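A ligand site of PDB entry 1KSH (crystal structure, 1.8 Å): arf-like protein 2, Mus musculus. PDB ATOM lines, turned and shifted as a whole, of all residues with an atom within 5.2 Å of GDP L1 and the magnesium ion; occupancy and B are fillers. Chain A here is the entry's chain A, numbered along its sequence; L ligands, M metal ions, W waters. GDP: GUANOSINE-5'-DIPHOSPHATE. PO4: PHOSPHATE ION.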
ATOM      1  N   LEU A  26     -25.232 -19.935  -9.836  1.00  0.00           N
ATOM      2  CA  LEU A  26     -26.206 -20.111  -8.771  1.00  0.00           C
ATOM      3  C   LEU A  26     -27.027 -18.852  -8.603  1.00  0.00           C
ATOM      4  O   LEU A  26     -26.613 -17.762  -9.017  1.00  0.00           O
ATOM      5  CB  LEU A  26     -25.494 -20.446  -7.458  1.00  0.00           C
ATOM      6  CG  LEU A  26     -24.554 -21.654  -7.536  1.00  0.00           C
ATOM      7  CD1 LEU A  26     -23.854 -21.830  -6.189  1.00  0.00           C
ATOM      8  CD2 LEU A  26     -25.335 -22.905  -7.915  1.00  0.00           C
ATOM      9  N   ASP A  27     -28.206 -18.996  -8.004  1.00  0.00           N
ATOM     10  CA  ASP A  27     -29.054 -17.847  -7.720  1.00  0.00           C
ATOM     11  C   ASP A  27     -28.265 -16.922  -6.798  1.00  0.00           C
ATOM     12  O   ASP A  27     -27.464 -17.389  -5.990  1.00  0.00           O
ATOM     13  CB  ASP A  27     -30.331 -18.309  -7.034  1.00  0.00           C
ATOM     14  CG  ASP A  27     -30.064 -19.160  -5.800  1.00  0.00           C
ATOM     15  OD1 ASP A  27     -29.427 -20.227  -5.937  1.00  0.00           O
ATOM     16  OD2 ASP A  27     -30.481 -18.764  -4.703  1.00  0.00           O
ATOM     17  N   ASN A  28     -28.475 -15.614  -6.931  1.00  0.00           N
ATOM     18  CA  ASN A  28     -27.787 -14.616  -6.112  1.00  0.00           C
ATOM     19  C   ASN A  28     -26.338 -14.340  -6.521  1.00  0.00           C
ATOM     20  O   ASN A  28     -25.663 -13.523  -5.891  1.00  0.00           O
ATOM     21  CB  ASN A  28     -27.849 -15.012  -4.631  1.00  0.00           C
ATOM     22  CG  ASN A  28     -27.443 -13.882  -3.697  1.00  0.00           C
ATOM     23  OD1 ASN A  28     -27.862 -12.728  -3.884  1.00  0.00           O
ATOM     24  ND2 ASN A  28     -26.643 -14.191  -2.686  1.00  0.00           N
ATOM     25  N   ALA A  29     -25.849 -15.002  -7.568  1.00  0.00           N
ATOM     26  CA  ALA A  29     -24.469 -14.768  -8.009  1.00  0.00           C
ATOM     27  C   ALA A  29     -24.309 -13.350  -8.577  1.00  0.00           C
ATOM     28  O   ALA A  29     -23.221 -12.776  -8.549  1.00  0.00           O
ATOM     29  CB  ALA A  29     -24.054 -15.809  -9.040  1.00  0.00           C
ATOM     30  N   GLY A  30     -25.401 -12.798  -9.087  1.00  0.00           N
ATOM     31  CA  GLY A  30     -25.357 -11.453  -9.640  1.00  0.00           C
ATOM     32  C   GLY A  30     -25.477 -11.385 -11.152  1.00  0.00           C
ATOM     33  O   GLY A  30     -25.126 -10.372 -11.756  1.00  0.00           O
ATOM     34  N   LYS A  31     -25.984 -12.459 -11.759  1.00  0.00           N
ATOM     35  CA  LYS A  31     -26.148 -12.524 -13.205  1.00  0.00           C
ATOM     36  C   LYS A  31     -26.938 -11.359 -13.784  1.00  0.00           C
ATOM     37  O   LYS A  31     -26.489 -10.683 -14.704  1.00  0.00           O
ATOM     38  CB  LYS A  31     -26.825 -13.847 -13.590  1.00  0.00           C
ATOM     39  CG  LYS A  31     -26.025 -15.088 -13.228  1.00  0.00           C
ATOM     40  CD  LYS A  31     -26.754 -16.384 -13.622  1.00  0.00           C
ATOM     41  CE  LYS A  31     -28.088 -16.561 -12.901  1.00  0.00           C
ATOM     42  NZ  LYS A  31     -27.925 -16.815 -11.428  1.00  0.00           N
ATOM     43  N   THR A  32     -28.129 -11.117 -13.244  1.00  0.00           N
ATOM     44  CA  THR A  32     -28.979 -10.044 -13.746  1.00  0.00           C
ATOM     45  C   THR A  32     -28.401  -8.657 -13.563  1.00  0.00           C
ATOM     46  O   THR A  32     -28.522  -7.803 -14.454  1.00  0.00           O
ATOM     47  CB  THR A  32     -30.366 -10.142 -13.104  1.00  0.00           C
ATOM     48  OG1 THR A  32     -30.882 -11.443 -13.377  1.00  0.00           O
ATOM     49  CG2 THR A  32     -31.332  -9.105 -13.661  1.00  0.00           C
ATOM     50  N   THR A  33     -27.752  -8.420 -12.429  1.00  0.00           N
ATOM     51  CA  THR A  33     -27.147  -7.118 -12.180  1.00  0.00           C
ATOM     52  C   THR A  33     -26.021  -6.884 -13.191  1.00  0.00           C
ATOM     53  O   THR A  33     -25.884  -5.792 -13.733  1.00  0.00           O
ATOM     54  CB  THR A  33     -26.598  -7.024 -10.731  1.00  0.00           C
ATOM     55  OG1 THR A  33     -27.666  -7.257  -9.808  1.00  0.00           O
ATOM     56  CG2 THR A  33     -26.011  -5.640 -10.466  1.00  0.00           C
ATOM     57  N   ILE A  34     -25.226  -7.923 -13.463  1.00  0.00           N
ATOM     58  CA  ILE A  34     -24.146  -7.784 -14.423  1.00  0.00           C
ATOM     59  C   ILE A  34     -24.710  -7.383 -15.787  1.00  0.00           C
ATOM     60  O   ILE A  34     -24.190  -6.490 -16.438  1.00  0.00           O
ATOM     61  CB  ILE A  34     -23.342  -9.095 -14.590  1.00  0.00           C
ATOM     62  CG1 ILE A  34     -22.477  -9.347 -13.349  1.00  0.00           C
ATOM     63  CG2 ILE A  34     -22.445  -9.030 -15.811  1.00  0.00           C
ATOM     64  CD1 ILE A  34     -21.669 -10.628 -13.417  1.00  0.00           C
ATOM     65  N   VAL A  43     -29.662  -0.765 -11.648  1.00  0.00           N
ATOM     66  CA  VAL A  43     -29.579  -2.075 -10.990  1.00  0.00           C
ATOM     67  C   VAL A  43     -29.921  -1.987  -9.505  1.00  0.00           C
ATOM     68  O   VAL A  43     -29.266  -2.617  -8.669  1.00  0.00           O
ATOM     69  CB  VAL A  43     -28.166  -2.675 -11.130  1.00  0.00           C
ATOM     70  CG1 VAL A  43     -27.808  -2.813 -12.606  1.00  0.00           C
ATOM     71  CG2 VAL A  43     -27.145  -1.808 -10.415  1.00  0.00           C
ATOM     72  N   ILE A  46     -33.616  -4.748  -8.924  1.00  0.00           N
ATOM     73  CA  ILE A  46     -33.469  -6.082  -9.505  1.00  0.00           C
ATOM     74  C   ILE A  46     -33.997  -7.158  -8.569  1.00  0.00           C
ATOM     75  O   ILE A  46     -33.627  -7.208  -7.391  1.00  0.00           O
ATOM     76  CB  ILE A  46     -31.979  -6.379  -9.834  1.00  0.00           C
ATOM     77  CG1 ILE A  46     -31.577  -5.615 -11.093  1.00  0.00           C
ATOM     78  CG2 ILE A  46     -31.765  -7.880 -10.008  1.00  0.00           C
ATOM     79  CD1 ILE A  46     -30.172  -5.898 -11.560  1.00  0.00           C
ATOM     80  N   SER A  47     -34.867  -8.016  -9.083  1.00  0.00           N
ATOM     81  CA  SER A  47     -35.442  -9.096  -8.291  1.00  0.00           C
ATOM     82  C   SER A  47     -35.038 -10.433  -8.898  1.00  0.00           C
ATOM     83  O   SER A  47     -34.475 -10.491  -9.992  1.00  0.00           O
ATOM     84  CB  SER A  47     -36.963  -8.965  -8.272  1.00  0.00           C
ATOM     85  OG  SER A  47     -37.482  -8.954  -9.590  1.00  0.00           O
ATOM     86  N   PRO A  48     -35.307 -11.541  -8.187  1.00  0.00           N
ATOM     87  CA  PRO A  48     -34.956 -12.857  -8.706  1.00  0.00           C
ATOM     88  C   PRO A  48     -35.570 -13.154 -10.066  1.00  0.00           C
ATOM     89  O   PRO A  48     -36.735 -12.842 -10.317  1.00  0.00           O
ATOM     90  CB  PRO A  48     -35.455 -13.797  -7.613  1.00  0.00           C
ATOM     91  CG  PRO A  48     -35.208 -13.011  -6.376  1.00  0.00           C
ATOM     92  CD  PRO A  48     -35.716 -11.633  -6.771  1.00  0.00           C
ATOM     93  N   THR A  49     -34.786 -13.773 -10.944  1.00  0.00           N
ATOM     94  CA  THR A  49     -35.263 -14.122 -12.278  1.00  0.00           C
ATOM     95  C   THR A  49     -35.943 -15.480 -12.201  1.00  0.00           C
ATOM     96  O   THR A  49     -35.318 -16.476 -11.828  1.00  0.00           O
ATOM     97  CB  THR A  49     -34.102 -14.183 -13.261  1.00  0.00           C
ATOM     98  OG1 THR A  49     -33.423 -12.918 -13.229  1.00  0.00           O
ATOM     99  CG2 THR A  49     -34.589 -14.449 -14.679  1.00  0.00           C
ATOM    100  N   ASN A  53     -33.918 -13.870 -18.919  1.00  0.00           N
ATOM    101  CA  ASN A  53     -33.816 -12.451 -19.258  1.00  0.00           C
ATOM    102  C   ASN A  53     -32.841 -12.438 -20.429  1.00  0.00           C
ATOM    103  O   ASN A  53     -31.673 -12.799 -20.283  1.00  0.00           O
ATOM    104  CB  ASN A  53     -33.223 -11.610 -18.117  1.00  0.00           C
ATOM    105  CG  ASN A  53     -34.225 -11.315 -17.007  1.00  0.00           C
ATOM    106  OD1 ASN A  53     -35.378 -10.974 -17.259  1.00  0.00           O
ATOM    107  ND2 ASN A  53     -33.770 -11.419 -15.761  1.00  0.00           N
ATOM    108  N   ASP A  68     -29.611 -14.618 -19.772  1.00  0.00           N
ATOM    109  CA  ASP A  68     -29.396 -14.686 -18.329  1.00  0.00           C
ATOM    110  C   ASP A  68     -30.531 -15.585 -17.836  1.00  0.00           C
ATOM    111  O   ASP A  68     -31.695 -15.182 -17.817  1.00  0.00           O
ATOM    112  CB  ASP A  68     -29.474 -13.277 -17.745  1.00  0.00           C
ATOM    113  CG  ASP A  68     -29.867 -13.245 -16.289  1.00  0.00           C
ATOM    114  OD1 ASP A  68     -29.601 -14.237 -15.580  1.00  0.00           O
ATOM    115  OD2 ASP A  68     -30.450 -12.215 -15.864  1.00  0.00           O
ATOM    116  N   ASN A 127     -17.698 -12.445  -9.312  1.00  0.00           N
ATOM    117  CA  ASN A 127     -18.435 -11.233  -8.977  1.00  0.00           C
ATOM    118  C   ASN A 127     -18.480 -10.863  -7.489  1.00  0.00           C
ATOM    119  O   ASN A 127     -18.116 -11.657  -6.623  1.00  0.00           O
ATOM    120  CB  ASN A 127     -19.862 -11.357  -9.543  1.00  0.00           C
ATOM    121  CG  ASN A 127     -20.628 -10.063  -9.501  1.00  0.00           C
ATOM    122  OD1 ASN A 127     -20.107  -9.014  -9.887  1.00  0.00           O
ATOM    123  ND2 ASN A 127     -21.880 -10.117  -9.069  1.00  0.00           N
ATOM    124  N   LYS A 128     -18.913  -9.637  -7.230  1.00  0.00           N
ATOM    125  CA  LYS A 128     -19.022  -9.088  -5.880  1.00  0.00           C
ATOM    126  C   LYS A 128     -17.655  -8.886  -5.227  1.00  0.00           C
ATOM    127  O   LYS A 128     -17.510  -9.060  -4.018  1.00  0.00           O
ATOM    128  CB  LYS A 128     -19.904  -9.984  -4.999  1.00  0.00           C
ATOM    129  CG  LYS A 128     -21.290 -10.220  -5.573  1.00  0.00           C
ATOM    130  CD  LYS A 128     -22.277 -10.701  -4.527  1.00  0.00           C
ATOM    131  CE  LYS A 128     -23.573 -11.175  -5.153  1.00  0.00           C
ATOM    132  NZ  LYS A 128     -24.603 -11.497  -4.137  1.00  0.00           N
ATOM    133  N   GLN A 129     -16.668  -8.525  -6.027  1.00  0.00           N
ATOM    134  CA  GLN A 129     -15.323  -8.291  -5.502  1.00  0.00           C
ATOM    135  C   GLN A 129     -15.291  -7.031  -4.633  1.00  0.00           C
ATOM    136  O   GLN A 129     -14.280  -6.707  -4.020  1.00  0.00           O
ATOM    137  CB  GLN A 129     -14.310  -8.174  -6.644  1.00  0.00           C
ATOM    138  CG  GLN A 129     -14.060  -9.498  -7.351  1.00  0.00           C
ATOM    139  CD  GLN A 129     -13.264 -10.472  -6.503  1.00  0.00           C
ATOM    140  OE1 GLN A 129     -13.587 -11.665  -6.439  1.00  0.00           O
ATOM    141  NE2 GLN A 129     -12.219  -9.974  -5.851  1.00  0.00           N
ATOM    142  N   ASP A 130     -16.404  -6.304  -4.607  1.00  0.00           N
ATOM    143  CA  ASP A 130     -16.508  -5.092  -3.808  1.00  0.00           C
ATOM    144  C   ASP A 130     -16.876  -5.457  -2.365  1.00  0.00           C
ATOM    145  O   ASP A 130     -16.930  -4.594  -1.498  1.00  0.00           O
ATOM    146  CB  ASP A 130     -17.599  -4.185  -4.354  1.00  0.00           C
ATOM    147  CG  ASP A 130     -18.941  -4.866  -4.381  1.00  0.00           C
ATOM    148  OD1 ASP A 130     -19.122  -5.758  -5.235  1.00  0.00           O
ATOM    149  OD2 ASP A 130     -19.796  -4.523  -3.550  1.00  0.00           O
ATOM    150  N   LEU A 131     -17.139  -6.742  -2.131  1.00  0.00           N
ATOM    151  CA  LEU A 131     -17.495  -7.205  -0.802  1.00  0.00           C
ATOM    152  C   LEU A 131     -16.260  -7.604   0.006  1.00  0.00           C
ATOM    153  O   LEU A 131     -15.299  -8.159  -0.545  1.00  0.00           O
ATOM    154  CB  LEU A 131     -18.456  -8.394  -0.876  1.00  0.00           C
ATOM    155  CG  LEU A 131     -19.889  -8.105  -1.337  1.00  0.00           C
ATOM    156  CD1 LEU A 131     -20.708  -9.383  -1.283  1.00  0.00           C
ATOM    157  CD2 LEU A 131     -20.510  -7.033  -0.460  1.00  0.00           C
ATOM    158  N   CYS A 159     -14.723  -9.127 -10.701  1.00  0.00           N
ATOM    159  CA  CYS A 159     -15.509  -7.944 -11.043  1.00  0.00           C
ATOM    160  C   CYS A 159     -16.520  -7.572  -9.974  1.00  0.00           C
ATOM    161  O   CYS A 159     -16.692  -8.273  -8.972  1.00  0.00           O
ATOM    162  CB  CYS A 159     -16.272  -8.191 -12.360  1.00  0.00           C
ATOM    163  SG  CYS A 159     -17.621  -9.426 -12.265  1.00  0.00           S
ATOM    164  N   SER A 160     -17.169  -6.435 -10.191  1.00  0.00           N
ATOM    165  CA  SER A 160     -18.211  -5.956  -9.292  1.00  0.00           C
ATOM    166  C   SER A 160     -19.355  -5.490 -10.182  1.00  0.00           C
ATOM    167  O   SER A 160     -19.212  -4.538 -10.949  1.00  0.00           O
ATOM    168  CB  SER A 160     -17.738  -4.799  -8.414  1.00  0.00           C
ATOM    169  OG  SER A 160     -18.787  -4.386  -7.553  1.00  0.00           O
ATOM    170  N   ALA A 161     -20.490  -6.173 -10.107  1.00  0.00           N
ATOM    171  CA  ALA A 161     -21.639  -5.818 -10.921  1.00  0.00           C
ATOM    172  C   ALA A 161     -22.304  -4.520 -10.454  1.00  0.00           C
ATOM    173  O   ALA A 161     -22.915  -3.814 -11.255  1.00  0.00           O
ATOM    174  CB  ALA A 161     -22.645  -6.961 -10.940  1.00  0.00           C
ATOM    175  N   VAL A 162     -22.184  -4.192  -9.165  1.00  0.00           N
ATOM    176  CA  VAL A 162     -22.800  -2.977  -8.651  1.00  0.00           C
ATOM    177  C   VAL A 162     -22.071  -1.706  -9.104  1.00  0.00           C
ATOM    178  O   VAL A 162     -22.708  -0.721  -9.451  1.00  0.00           O
ATOM    179  CB  VAL A 162     -22.878  -2.969  -7.096  1.00  0.00           C
ATOM    180  CG1 VAL A 162     -23.850  -4.032  -6.642  1.00  0.00           C
ATOM    181  CG2 VAL A 162     -21.512  -3.203  -6.493  1.00  0.00           C
HETATM  182  PB  GDP L   1     -28.817 -13.343  -9.925  1.00  0.00           P
HETATM  183  O1B GDP L   1     -29.574 -12.865 -11.096  1.00  0.00           O
HETATM  184  O2B GDP L   1     -29.596 -14.238  -8.955  1.00  0.00           O
HETATM  185  O3B GDP L   1     -27.551 -14.182 -10.100  1.00  0.00           O
HETATM  186  O3A GDP L   1     -28.509 -12.171  -8.915  1.00  0.00           O
HETATM  187  PA  GDP L   1     -28.840 -10.735  -8.888  1.00  0.00           P
HETATM  188  O1A GDP L   1     -28.241  -9.985 -10.073  1.00  0.00           O
HETATM  189  O2A GDP L   1     -30.338 -10.529  -8.987  1.00  0.00           O
HETATM  190  O5' GDP L   1     -28.217 -10.265  -7.596  1.00  0.00           O
HETATM  191  C5' GDP L   1     -28.624 -10.792  -6.341  1.00  0.00           C
HETATM  192  C4' GDP L   1     -28.324  -9.755  -5.192  1.00  0.00           C
HETATM  193  O4' GDP L   1     -26.941  -9.517  -5.147  1.00  0.00           O
HETATM  194  C3' GDP L   1     -29.024  -8.398  -5.418  1.00  0.00           C
HETATM  195  O3' GDP L   1     -29.362  -7.990  -4.069  1.00  0.00           O
HETATM  196  C2' GDP L   1     -27.916  -7.536  -6.013  1.00  0.00           C
HETATM  197  O2' GDP L   1     -28.025  -6.117  -5.826  1.00  0.00           O
HETATM  198  C1' GDP L   1     -26.661  -8.122  -5.343  1.00  0.00           C
HETATM  199  N9  GDP L   1     -25.475  -8.053  -6.223  1.00  0.00           N
HETATM  200  C8  GDP L   1     -25.293  -8.510  -7.537  1.00  0.00           C
HETATM  201  N7  GDP L   1     -24.059  -8.276  -7.985  1.00  0.00           N
HETATM  202  C5  GDP L   1     -23.358  -7.614  -6.908  1.00  0.00           C
HETATM  203  C6  GDP L   1     -21.946  -7.050  -6.674  1.00  0.00           C
HETATM  204  O6  GDP L   1     -21.079  -7.110  -7.530  1.00  0.00           O
HETATM  205  N1  GDP L   1     -21.575  -6.451  -5.485  1.00  0.00           N
HETATM  206  C2  GDP L   1     -22.461  -6.318  -4.397  1.00  0.00           C
HETATM  207  N2  GDP L   1     -22.083  -5.733  -3.256  1.00  0.00           N
HETATM  208  N3  GDP L   1     -23.755  -6.828  -4.606  1.00  0.00           N
HETATM  209  C4  GDP L   1     -24.207  -7.493  -5.868  1.00  0.00           C
HETATM  210  P   PO4 L   2     -31.695 -15.844 -10.100  1.00  0.00           P
HETATM  211  O1  PO4 L   2     -32.033 -14.502 -10.578  1.00  0.00           O
HETATM  212  O2  PO4 L   2     -31.470 -15.799  -8.638  1.00  0.00           O
HETATM  213  O3  PO4 L   2     -30.464 -16.314 -10.780  1.00  0.00           O
HETATM  214  O4  PO4 L   2     -32.831 -16.778 -10.378  1.00  0.00           O
HETATM  215 MG    MG M   1     -31.513 -12.975 -12.085  1.00  0.00          MG
HETATM  216  O   HOH W   1     -32.666 -10.701  -7.020  1.00  0.00           O
HETATM  217  O   HOH W   2     -28.327  -5.085  -8.376  1.00  0.00           O
HETATM  218  O   HOH W   3     -30.805 -14.544 -13.358  1.00  0.00           O
HETATM  219  O   HOH W   4     -31.410 -13.009  -6.671  1.00  0.00           O
HETATM  220  O   HOH W   5     -32.271 -11.270 -10.723  1.00  0.00           O
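The side-chain amino group (NZ) of Lys 128 lies within hydrogen-bond range of an oxygen (O4') of GDP L1, at 3.2 Å.
OD1 of Asp 130 sits at hydrogen-bond distance from N1 of GDP L1 (2.6 Å).
The backbone NH (N) of Gly 30 is in hydrogen-bond range of an oxygen (O3B) of GDP L1, at 2.8 Å.
NZ of Lys 31 is in salt-bridge range of O3B of GDP L1 (3.0 Å).
The backbone NH (N) of Thr 32 is in hydrogen-bond range of an oxygen (O1A) of GDP L1 (3.4 Å).
An oxygen (O2B) of GDP L1 sits at hydrogen-bond distance from the backbone NH of Asn 28, 2.7 Å away.
N of Ala 161 lies within hydrogen-bond range of O6 of GDP L1 (2.8 Å).
The backbone NH of Lys 128 lies close to an oxygen (O6) of GDP L1 (3.3 Å).
ND2 of Asn 127 sits at hydrogen-bond distance from N7 of GDP L1, at 3.1 Å.
O1A of GDP L1 is in hydrogen-bond range of OG1 of Thr 33, at 2.8 Å.
O1A of GDP L1 sits at hydrogen-bond distance from N of Thr 33, at 2.9 Å.
The backbone NH (N) of Ala 29 lies within hydrogen-bond range of an oxygen (O3B) of GDP L1, 3.2 Å away.
The backbone NH (N) of Lys 31 is in hydrogen-bond range of an oxygen (O3B) of GDP L1, at 2.9 Å.
N of Asp 68 lies within hydrogen-bond range of O of Asn 53 (2.8 Å).
O of Leu 26 is in hydrogen-bond range of NZ of Lys 31.
OD2 of Asp 68 lies close to OG1 of Thr 32 (2.6 Å).
O of Ala 29 sits at hydrogen-bond distance from ND2 of Asn 127 (3.0 Å).
The backbone NH of Lys 128 sits at hydrogen-bond distance from the backbone carbonyl oxygen of Cys 159 (3.1 Å).
The side-chain amide oxygen (OD1) of Asn 127 is in hydrogen-bond range of the backbone NH (N) of Ala 161.
SG of Cys 159 sits at hydrogen-bond distance from OD1 of Asn 127 (3.5 Å).
The side-chain hydroxyl of Thr 49 sits close to the side-chain amide nitrogen of Asn 53 (3.0 Å).
Residues that only touch GDP L1: Ile 46 (3.2 Å), Val 162 (3.4 Å), Leu 131 (3.5 Å), Ser 160 (3.6 Å), Asp 27 (3.7 Å) and Leu 26 (3.9 Å).
Hydrophobic or aromatic side chains within 4 Å of GDP L1: Ala 29, Ile 46, Leu 131, Ala 161 and Val 162.
Within 4 Å of GDP L1: Leu 26, Asp 27, Asn 28, Ala 29, Gly 30, Lys 31, Thr 32, Thr 33, Ile 46, Asn 127, Lys 128, Asp 130, Leu 131, Ser 160, Ala 161 and Val 162.
Along chain A the residues within 4 Å of GDP L1 span positions 26 to 162.
The nearest printed residue that does not touch GDP L1 is Ser 47 (4.3 Å).
Merely in contact with the magnesium ion: Asp 68.
Three residues have an atom within 4 Å of the magnesium ion: Thr 32, Thr 49 and Asp 68.
The nearest printed residue that does not touch the magnesium ion is Ser 47 (4.4 Å).
The magnesium ion is bound by OG1 of Thr 32 (2.1 Å), water W3 (2.1 Å), O1B of GDP L1 (2.2 Å), O1 of PO4 L2 (2.2 Å), OG1 of Thr 49 (2.2 Å) and water W5 (2.3 Å).
Water W5 bridges the backbone carbonyl oxygen of Ser 47 (2.4 Å) and an oxygen (O2A) of GDP L1 (2.7 Å).
Water W2 lies within hydrogen-bond range of the backbone carbonyl oxygen of Val 43 (2.7 Å), the side-chain hydroxyl of Thr 33 (2.7 Å) and an oxygen (O2') of GDP L1 (2.8 Å).
Water W1 lies within hydrogen-bond range of O2A of GDP L1 (3.1 Å) and O of Ser 47 (3.5 Å).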
